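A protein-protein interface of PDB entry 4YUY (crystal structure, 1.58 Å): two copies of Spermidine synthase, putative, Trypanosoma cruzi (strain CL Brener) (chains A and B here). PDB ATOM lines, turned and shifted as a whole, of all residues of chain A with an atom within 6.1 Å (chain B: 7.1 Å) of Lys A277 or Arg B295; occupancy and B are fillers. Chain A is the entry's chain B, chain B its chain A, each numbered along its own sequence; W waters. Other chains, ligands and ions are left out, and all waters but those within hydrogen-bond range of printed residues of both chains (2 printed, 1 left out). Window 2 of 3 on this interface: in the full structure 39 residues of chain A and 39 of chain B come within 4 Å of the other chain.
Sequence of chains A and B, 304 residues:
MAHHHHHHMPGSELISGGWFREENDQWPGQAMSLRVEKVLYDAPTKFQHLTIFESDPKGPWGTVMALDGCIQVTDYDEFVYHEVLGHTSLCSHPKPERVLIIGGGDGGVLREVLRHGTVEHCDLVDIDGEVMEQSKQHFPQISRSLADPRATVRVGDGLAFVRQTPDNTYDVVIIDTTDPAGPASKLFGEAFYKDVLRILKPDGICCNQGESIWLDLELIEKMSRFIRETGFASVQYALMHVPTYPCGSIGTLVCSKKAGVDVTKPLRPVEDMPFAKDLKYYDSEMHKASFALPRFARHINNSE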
ATOM      1  N   GLU A 271      11.613 -12.990 -17.213  1.00  0.00           N
ATOM      2  CA  GLU A 271      12.992 -13.130 -17.666  1.00  0.00           C
ATOM      3  C   GLU A 271      13.536 -11.791 -18.130  1.00  0.00           C
ATOM      4  O   GLU A 271      14.750 -11.643 -18.084  1.00  0.00           O
ATOM      5  CB  GLU A 271      13.131 -14.124 -18.823  1.00  0.00           C
ATOM      6  CG  GLU A 271      12.879 -15.606 -18.509  1.00  0.00           C
ATOM      7  CD  GLU A 271      11.413 -15.914 -18.216  1.00  0.00           C
ATOM      8  OE1 GLU A 271      10.493 -15.271 -18.758  1.00  0.00           O
ATOM      9  OE2 GLU A 271      11.238 -16.879 -17.484  1.00  0.00           O
ATOM     10  N   MET A 273      13.102  -9.050 -16.367  1.00  0.00           N
ATOM     11  CA  MET A 273      13.119  -8.300 -15.145  1.00  0.00           C
ATOM     12  C   MET A 273      14.349  -8.719 -14.374  1.00  0.00           C
ATOM     13  O   MET A 273      14.837  -9.873 -14.515  1.00  0.00           O
ATOM     14  CB  MET A 273      11.844  -8.603 -14.349  1.00  0.00           C
ATOM     15  CG  MET A 273      10.611  -8.319 -15.187  1.00  0.00           C
ATOM     16  SD  MET A 273       9.113  -8.482 -14.159  1.00  0.00           S
ATOM     17  CE  MET A 273       7.869  -8.235 -15.383  1.00  0.00           C
ATOM     18  N   PRO A 274      14.902  -7.821 -13.574  1.00  0.00           N
ATOM     19  CA  PRO A 274      16.198  -8.041 -12.981  1.00  0.00           C
ATOM     20  C   PRO A 274      16.245  -9.081 -11.873  1.00  0.00           C
ATOM     21  O   PRO A 274      17.311  -9.609 -11.544  1.00  0.00           O
ATOM     22  CB  PRO A 274      16.590  -6.628 -12.441  1.00  0.00           C
ATOM     23  CG  PRO A 274      15.318  -5.882 -12.356  1.00  0.00           C
ATOM     24  CD  PRO A 274      14.468  -6.417 -13.460  1.00  0.00           C
ATOM     25  N   PHE A 275      15.065  -9.458 -11.380  1.00  0.00           N
ATOM     26  CA  PHE A 275      14.976 -10.386 -10.230  1.00  0.00           C
ATOM     27  C   PHE A 275      14.595 -11.842 -10.647  1.00  0.00           C
ATOM     28  O   PHE A 275      14.428 -12.684  -9.756  1.00  0.00           O
ATOM     29  CB  PHE A 275      13.915  -9.847  -9.207  1.00  0.00           C
ATOM     30  CG  PHE A 275      12.510  -9.736  -9.776  1.00  0.00           C
ATOM     31  CD1 PHE A 275      11.679 -10.887  -9.821  1.00  0.00           C
ATOM     32  CD2 PHE A 275      12.055  -8.497 -10.279  1.00  0.00           C
ATOM     33  CE1 PHE A 275      10.389 -10.801 -10.342  1.00  0.00           C
ATOM     34  CE2 PHE A 275      10.774  -8.398 -10.792  1.00  0.00           C
ATOM     35  CZ  PHE A 275       9.942  -9.550 -10.807  1.00  0.00           C
ATOM     36  N   ALA A 276      14.458 -12.122 -11.949  1.00  0.00           N
ATOM     37  CA  ALA A 276      14.025 -13.485 -12.390  1.00  0.00           C
ATOM     38  C   ALA A 276      14.929 -14.576 -11.838  1.00  0.00           C
ATOM     39  O   ALA A 276      14.444 -15.602 -11.406  1.00  0.00           O
ATOM     40  CB  ALA A 276      14.001 -13.559 -13.919  1.00  0.00           C
ATOM     41  N   LYS A 277      16.247 -14.270 -11.741  1.00  0.00           N
ATOM     42  CA  LYS A 277      17.202 -15.275 -11.222  1.00  0.00           C
ATOM     43  C   LYS A 277      17.133 -15.521  -9.759  1.00  0.00           C
ATOM     44  O   LYS A 277      17.671 -16.506  -9.309  1.00  0.00           O
ATOM     45  CB  LYS A 277      18.617 -14.932 -11.691  1.00  0.00           C
ATOM     46  CG  LYS A 277      18.675 -15.020 -13.186  1.00  0.00           C
ATOM     47  CD  LYS A 277      19.759 -14.090 -13.725  1.00  0.00           C
ATOM     48  CE  LYS A 277      20.023 -14.413 -15.197  1.00  0.00           C
ATOM     49  NZ  LYS A 277      18.728 -14.588 -15.918  1.00  0.00           N
ATOM     50  N   ASP A 278      16.429 -14.666  -8.999  1.00  0.00           N
ATOM     51  CA  ASP A 278      16.332 -14.844  -7.575  1.00  0.00           C
ATOM     52  C   ASP A 278      15.169 -15.772  -7.237  1.00  0.00           C
ATOM     53  O   ASP A 278      15.017 -16.182  -6.056  1.00  0.00           O
ATOM     54  CB  ASP A 278      16.118 -13.496  -6.878  1.00  0.00           C
ATOM     55  CG  ASP A 278      17.227 -12.510  -7.148  1.00  0.00           C
ATOM     56  OD1 ASP A 278      18.386 -12.962  -7.238  1.00  0.00           O
ATOM     57  OD2 ASP A 278      16.874 -11.296  -7.194  1.00  0.00           O
ATOM     58  N   LEU A 279      14.330 -16.068  -8.229  1.00  0.00           N
ATOM     59  CA  LEU A 279      13.113 -16.885  -7.861  1.00  0.00           C
ATOM     60  C   LEU A 279      13.458 -18.369  -7.810  1.00  0.00           C
ATOM     61  O   LEU A 279      14.278 -18.846  -8.563  1.00  0.00           O
ATOM     62  CB  LEU A 279      12.021 -16.667  -8.934  1.00  0.00           C
ATOM     63  CG  LEU A 279      11.546 -15.178  -9.058  1.00  0.00           C
ATOM     64  CD1 LEU A 279      10.360 -15.114  -9.993  1.00  0.00           C
ATOM     65  CD2 LEU A 279      11.240 -14.421  -7.750  1.00  0.00           C
ATOM     66  N   LYS A 280      12.712 -19.119  -6.997  1.00  0.00           N
ATOM     67  CA  LYS A 280      13.019 -20.494  -6.741  1.00  0.00           C
ATOM     68  C   LYS A 280      12.031 -21.484  -7.422  1.00  0.00           C
ATOM     69  O   LYS A 280      12.323 -22.706  -7.574  1.00  0.00           O
ATOM     70  CB  LYS A 280      12.997 -20.728  -5.242  1.00  0.00           C
ATOM     71  CG  LYS A 280      14.240 -20.141  -4.500  1.00  0.00           C
ATOM     72  CD  LYS A 280      14.020 -20.230  -2.983  1.00  0.00           C
ATOM     73  CE  LYS A 280      14.945 -19.330  -2.158  1.00  0.00           C
ATOM     74  NZ  LYS A 280      14.172 -18.637  -1.080  1.00  0.00           N
ATOM     75  N   TYR A 281      10.868 -20.953  -7.868  1.00  0.00           N
ATOM     76  CA  TYR A 281       9.891 -21.761  -8.510  1.00  0.00           C
ATOM     77  C   TYR A 281       9.495 -21.179  -9.845  1.00  0.00           C
ATOM     78  O   TYR A 281       9.671 -21.850 -10.884  1.00  0.00           O
ATOM     79  CB  TYR A 281       8.659 -21.854  -7.602  1.00  0.00           C
ATOM     80  CG  TYR A 281       7.547 -22.784  -8.109  1.00  0.00           C
ATOM     81  CD1 TYR A 281       7.540 -24.121  -7.738  1.00  0.00           C
ATOM     82  CD2 TYR A 281       6.542 -22.305  -8.915  1.00  0.00           C
ATOM     83  CE1 TYR A 281       6.467 -24.982  -8.143  1.00  0.00           C
ATOM     84  CE2 TYR A 281       5.475 -23.131  -9.322  1.00  0.00           C
ATOM     85  CZ  TYR A 281       5.450 -24.494  -8.965  1.00  0.00           C
ATOM     86  OH  TYR A 281       4.392 -25.319  -9.340  1.00  0.00           O
ATOM     87  N   TYR A 282       8.970 -19.943  -9.834  1.00  0.00           N
ATOM     88  CA  TYR A 282       8.362 -19.290 -10.972  1.00  0.00           C
ATOM     89  C   TYR A 282       9.290 -18.871 -12.103  1.00  0.00           C
ATOM     90  O   TYR A 282      10.352 -18.298 -11.879  1.00  0.00           O
ATOM     91  CB  TYR A 282       7.473 -18.060 -10.439  1.00  0.00           C
ATOM     92  CG  TYR A 282       6.800 -17.315 -11.605  1.00  0.00           C
ATOM     93  CD1 TYR A 282       7.457 -16.382 -12.309  1.00  0.00           C
ATOM     94  CD2 TYR A 282       5.438 -17.524 -11.930  1.00  0.00           C
ATOM     95  CE1 TYR A 282       6.856 -15.747 -13.364  1.00  0.00           C
ATOM     96  CE2 TYR A 282       4.833 -16.962 -13.017  1.00  0.00           C
ATOM     97  CZ  TYR A 282       5.547 -16.048 -13.740  1.00  0.00           C
ATOM     98  OH  TYR A 282       4.918 -15.368 -14.741  1.00  0.00           O
ATOM     99  N   ASP A 283       8.854 -19.105 -13.299  1.00  0.00           N
ATOM    100  CA  ASP A 283       9.416 -18.495 -14.524  1.00  0.00           C
ATOM    101  C   ASP A 283       8.387 -18.631 -15.606  1.00  0.00           C
ATOM    102  O   ASP A 283       7.292 -19.099 -15.362  1.00  0.00           O
ATOM    103  CB  ASP A 283      10.796 -19.157 -14.895  1.00  0.00           C
ATOM    104  CG  ASP A 283      10.723 -20.625 -15.327  1.00  0.00           C
ATOM    105  OD1 ASP A 283       9.641 -21.177 -15.643  1.00  0.00           O
ATOM    106  OD2 ASP A 283      11.808 -21.240 -15.376  1.00  0.00           O
ATOM    107  N   MET A 286       7.049 -22.110 -16.367  1.00  0.00           N
ATOM    108  CA  MET A 286       6.188 -22.597 -15.283  1.00  0.00           C
ATOM    109  C   MET A 286       4.859 -21.842 -15.321  1.00  0.00           C
ATOM    110  O   MET A 286       3.762 -22.506 -15.107  1.00  0.00           O
ATOM    111  CB  MET A 286       6.848 -22.410 -13.933  1.00  0.00           C
ATOM    112  CG  MET A 286       7.922 -23.406 -13.502  1.00  0.00           C
ATOM    113  SD  MET A 286       7.279 -25.101 -13.620  1.00  0.00           S
ATOM    114  CE  MET A 286       6.583 -25.438 -12.055  1.00  0.00           C
ATOM    115  N   LEU B 293       9.790 -27.476 -15.183  1.00  0.00           N
ATOM    116  CA  LEU B 293      10.080 -27.832 -13.781  1.00  0.00           C
ATOM    117  C   LEU B 293      10.303 -26.517 -13.020  1.00  0.00           C
ATOM    118  O   LEU B 293      10.776 -25.555 -13.657  1.00  0.00           O
ATOM    119  CB  LEU B 293      11.412 -28.618 -13.672  1.00  0.00           C
ATOM    120  CG  LEU B 293      11.341 -29.956 -14.424  1.00  0.00           C
ATOM    121  CD1 LEU B 293      12.626 -30.749 -14.242  1.00  0.00           C
ATOM    122  CD2 LEU B 293      10.157 -30.828 -13.970  1.00  0.00           C
ATOM    123  N   PRO B 294      10.064 -26.527 -11.711  1.00  0.00           N
ATOM    124  CA  PRO B 294      10.304 -25.325 -10.859  1.00  0.00           C
ATOM    125  C   PRO B 294      11.793 -24.931 -11.022  1.00  0.00           C
ATOM    126  O   PRO B 294      12.649 -25.799 -11.254  1.00  0.00           O
ATOM    127  CB  PRO B 294      10.121 -25.854  -9.453  1.00  0.00           C
ATOM    128  CG  PRO B 294       9.171 -26.989  -9.574  1.00  0.00           C
ATOM    129  CD  PRO B 294       9.416 -27.607 -10.930  1.00  0.00           C
ATOM    130  N   ARG B 295      12.093 -23.654 -10.945  1.00  0.00           N
ATOM    131  CA  ARG B 295      13.489 -23.233 -11.108  1.00  0.00           C
ATOM    132  C   ARG B 295      14.509 -24.035 -10.284  1.00  0.00           C
ATOM    133  O   ARG B 295      15.576 -24.376 -10.808  1.00  0.00           O
ATOM    134  CB  ARG B 295      13.564 -21.709 -10.815  1.00  0.00           C
ATOM    135  CG  ARG B 295      13.328 -20.854 -12.062  1.00  0.00           C
ATOM    136  CD  ARG B 295      13.584 -19.369 -11.831  1.00  0.00           C
ATOM    137  NE  ARG B 295      14.877 -19.110 -11.219  1.00  0.00           N
ATOM    138  CZ  ARG B 295      16.024 -19.031 -11.852  1.00  0.00           C
ATOM    139  NH1 ARG B 295      16.104 -19.267 -13.176  1.00  0.00           N
ATOM    140  NH2 ARG B 295      17.072 -18.817 -11.128  1.00  0.00           N
ATOM    141  N   PHE B 296      14.207 -24.414  -9.038  1.00  0.00           N
ATOM    142  CA  PHE B 296      15.154 -25.169  -8.235  1.00  0.00           C
ATOM    143  C   PHE B 296      15.529 -26.549  -8.777  1.00  0.00           C
ATOM    144  O   PHE B 296      16.561 -27.125  -8.364  1.00  0.00           O
ATOM    145  CB  PHE B 296      14.698 -25.288  -6.775  1.00  0.00           C
ATOM    146  CG  PHE B 296      13.551 -26.186  -6.490  1.00  0.00           C
ATOM    147  CD1 PHE B 296      13.801 -27.579  -6.302  1.00  0.00           C
ATOM    148  CD2 PHE B 296      12.241 -25.734  -6.374  1.00  0.00           C
ATOM    149  CE1 PHE B 296      12.780 -28.445  -5.996  1.00  0.00           C
ATOM    150  CE2 PHE B 296      11.212 -26.630  -6.069  1.00  0.00           C
ATOM    151  CZ  PHE B 296      11.482 -28.001  -5.888  1.00  0.00           C
ATOM    152  N   ALA B 297      14.630 -27.100  -9.602  1.00  0.00           N
ATOM    153  CA  ALA B 297      14.889 -28.421 -10.232  1.00  0.00           C
ATOM    154  C   ALA B 297      15.220 -28.379 -11.701  1.00  0.00           C
ATOM    155  O   ALA B 297      15.454 -29.471 -12.288  1.00  0.00           O
ATOM    156  CB  ALA B 297      13.622 -29.301 -10.052  1.00  0.00           C
ATOM    157  N   ARG B 298      15.279 -27.191 -12.309  1.00  0.00           N
ATOM    158  CA  ARG B 298      15.233 -27.033 -13.817  1.00  0.00           C
ATOM    159  C   ARG B 298      16.417 -27.687 -14.434  1.00  0.00           C
ATOM    160  O   ARG B 298      16.358 -28.014 -15.579  1.00  0.00           O
ATOM    161  CB  ARG B 298      15.106 -25.560 -14.259  1.00  0.00           C
ATOM    162  CG  ARG B 298      16.392 -24.784 -13.984  1.00  0.00           C
ATOM    163  CD  ARG B 298      16.214 -23.313 -14.404  1.00  0.00           C
ATOM    164  NE  ARG B 298      17.455 -22.552 -14.214  1.00  0.00           N
ATOM    165  CZ  ARG B 298      17.930 -22.132 -13.039  1.00  0.00           C
ATOM    166  NH1 ARG B 298      17.293 -22.352 -11.885  1.00  0.00           N
ATOM    167  NH2 ARG B 298      19.065 -21.467 -13.024  1.00  0.00           N
ATOM    168  N   HIS B 299      17.516 -27.788 -13.685  1.00  0.00           N
ATOM    169  CA  HIS B 299      18.769 -28.265 -14.230  1.00  0.00           C
ATOM    170  C   HIS B 299      18.680 -29.734 -14.665  1.00  0.00           C
ATOM    171  O   HIS B 299      19.532 -30.185 -15.415  1.00  0.00           O
ATOM    172  CB  HIS B 299      19.917 -28.071 -13.205  1.00  0.00           C
ATOM    173  CG  HIS B 299      19.674 -28.691 -11.853  1.00  0.00           C
ATOM    174  ND1 HIS B 299      18.814 -28.111 -10.942  1.00  0.00           N
ATOM    175  CD2 HIS B 299      20.186 -29.774 -11.242  1.00  0.00           C
ATOM    176  CE1 HIS B 299      18.820 -28.814  -9.818  1.00  0.00           C
ATOM    177  NE2 HIS B 299      19.623 -29.857  -9.989  1.00  0.00           N
HETATM  178  O   HOH W   1      14.120 -19.746 -15.379  1.00  0.00           O
HETATM  179  O   HOH W   2      12.800 -23.703 -14.436  1.00  0.00           O
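Water W1 lies within hydrogen-bond range of the side-chain carboxylate of Asp A283 (2.8 Å) and the guanidinium group of Arg B295 (3.0 Å).
Water W2 bridges the side-chain carboxylate (OD2) of Asp A283 (2.8 Å) and the backbone carbonyl oxygen (O) of Leu B293 (2.9 Å).
No position is printed for both chains.
The guanidinium group (NE) of Arg B295 lies within hydrogen-bond range of the backbone carbonyl oxygen (O) of Leu A279 (2.7 Å).
N of Arg B295 lies within hydrogen-bond range of O of Tyr A281 (3.0 Å).
The side-chain sulfur of Met A286 sits close to the backbone NH of Leu B293.
O of Lys A277 is in hydrogen-bond range of NH2 of Arg B295 (3.0 Å).
N of Phe B296 is in hydrogen-bond range of O of Lys A280 (2.9 Å).
The side-chain sulfur of Met A286 lies close to the backbone nitrogen of Pro B294 (3.7 Å).
Lys A277 touches just one residue of chain B: Arg B295 (3.0 Å).
Of the printed residues of chain B, Tyr A281 touches Pro B294 (3.5 Å) and Arg B295 (3.0 Å).
Of the printed residues of chain B, Tyr A282 touches Arg B295.
Arg B295 touches seven residues of chain A.
Arg B298 touches none of the printed residues of chain A.
The nearest residue of chain B that does not touch Lys A277 is Arg B298 (6.4 Å).
The nearest residue of chain A that does not touch Arg B295 is Asp A278 (4.7 Å).
The nearest printed residue of chain B that does not touch Tyr A281 is Phe B296 (4.8 Å).
The backbone carbonyl oxygen (O) of Arg B295 lies within hydrogen-bond range of the guanidinium group (NH1) of Arg B298, at 2.9 Å.
OD1 of Asp A283 sits at hydrogen-bond distance from N of Met A286 (2.8 Å).
O of Ala A276 touches NE of Arg B295, 3.5 Å away.
O of Lys A280 touches N of Arg B295, 3.5 Å away.
CA of Pro B294 touches O of Tyr A281, at 3.5 Å.
Arg B295 touches Tyr A282.
Arg B295 touches Asp A283.
Along chain B the printed residues that touch a printed residue of chain A span positions 293 to 296.
Among the printed residues, 11 pairs touch across the chains.
Among the printed residues, no Asp or Glu carboxylate lies within 4 Å of a Lys or Arg side-chain nitrogen of the other chain.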
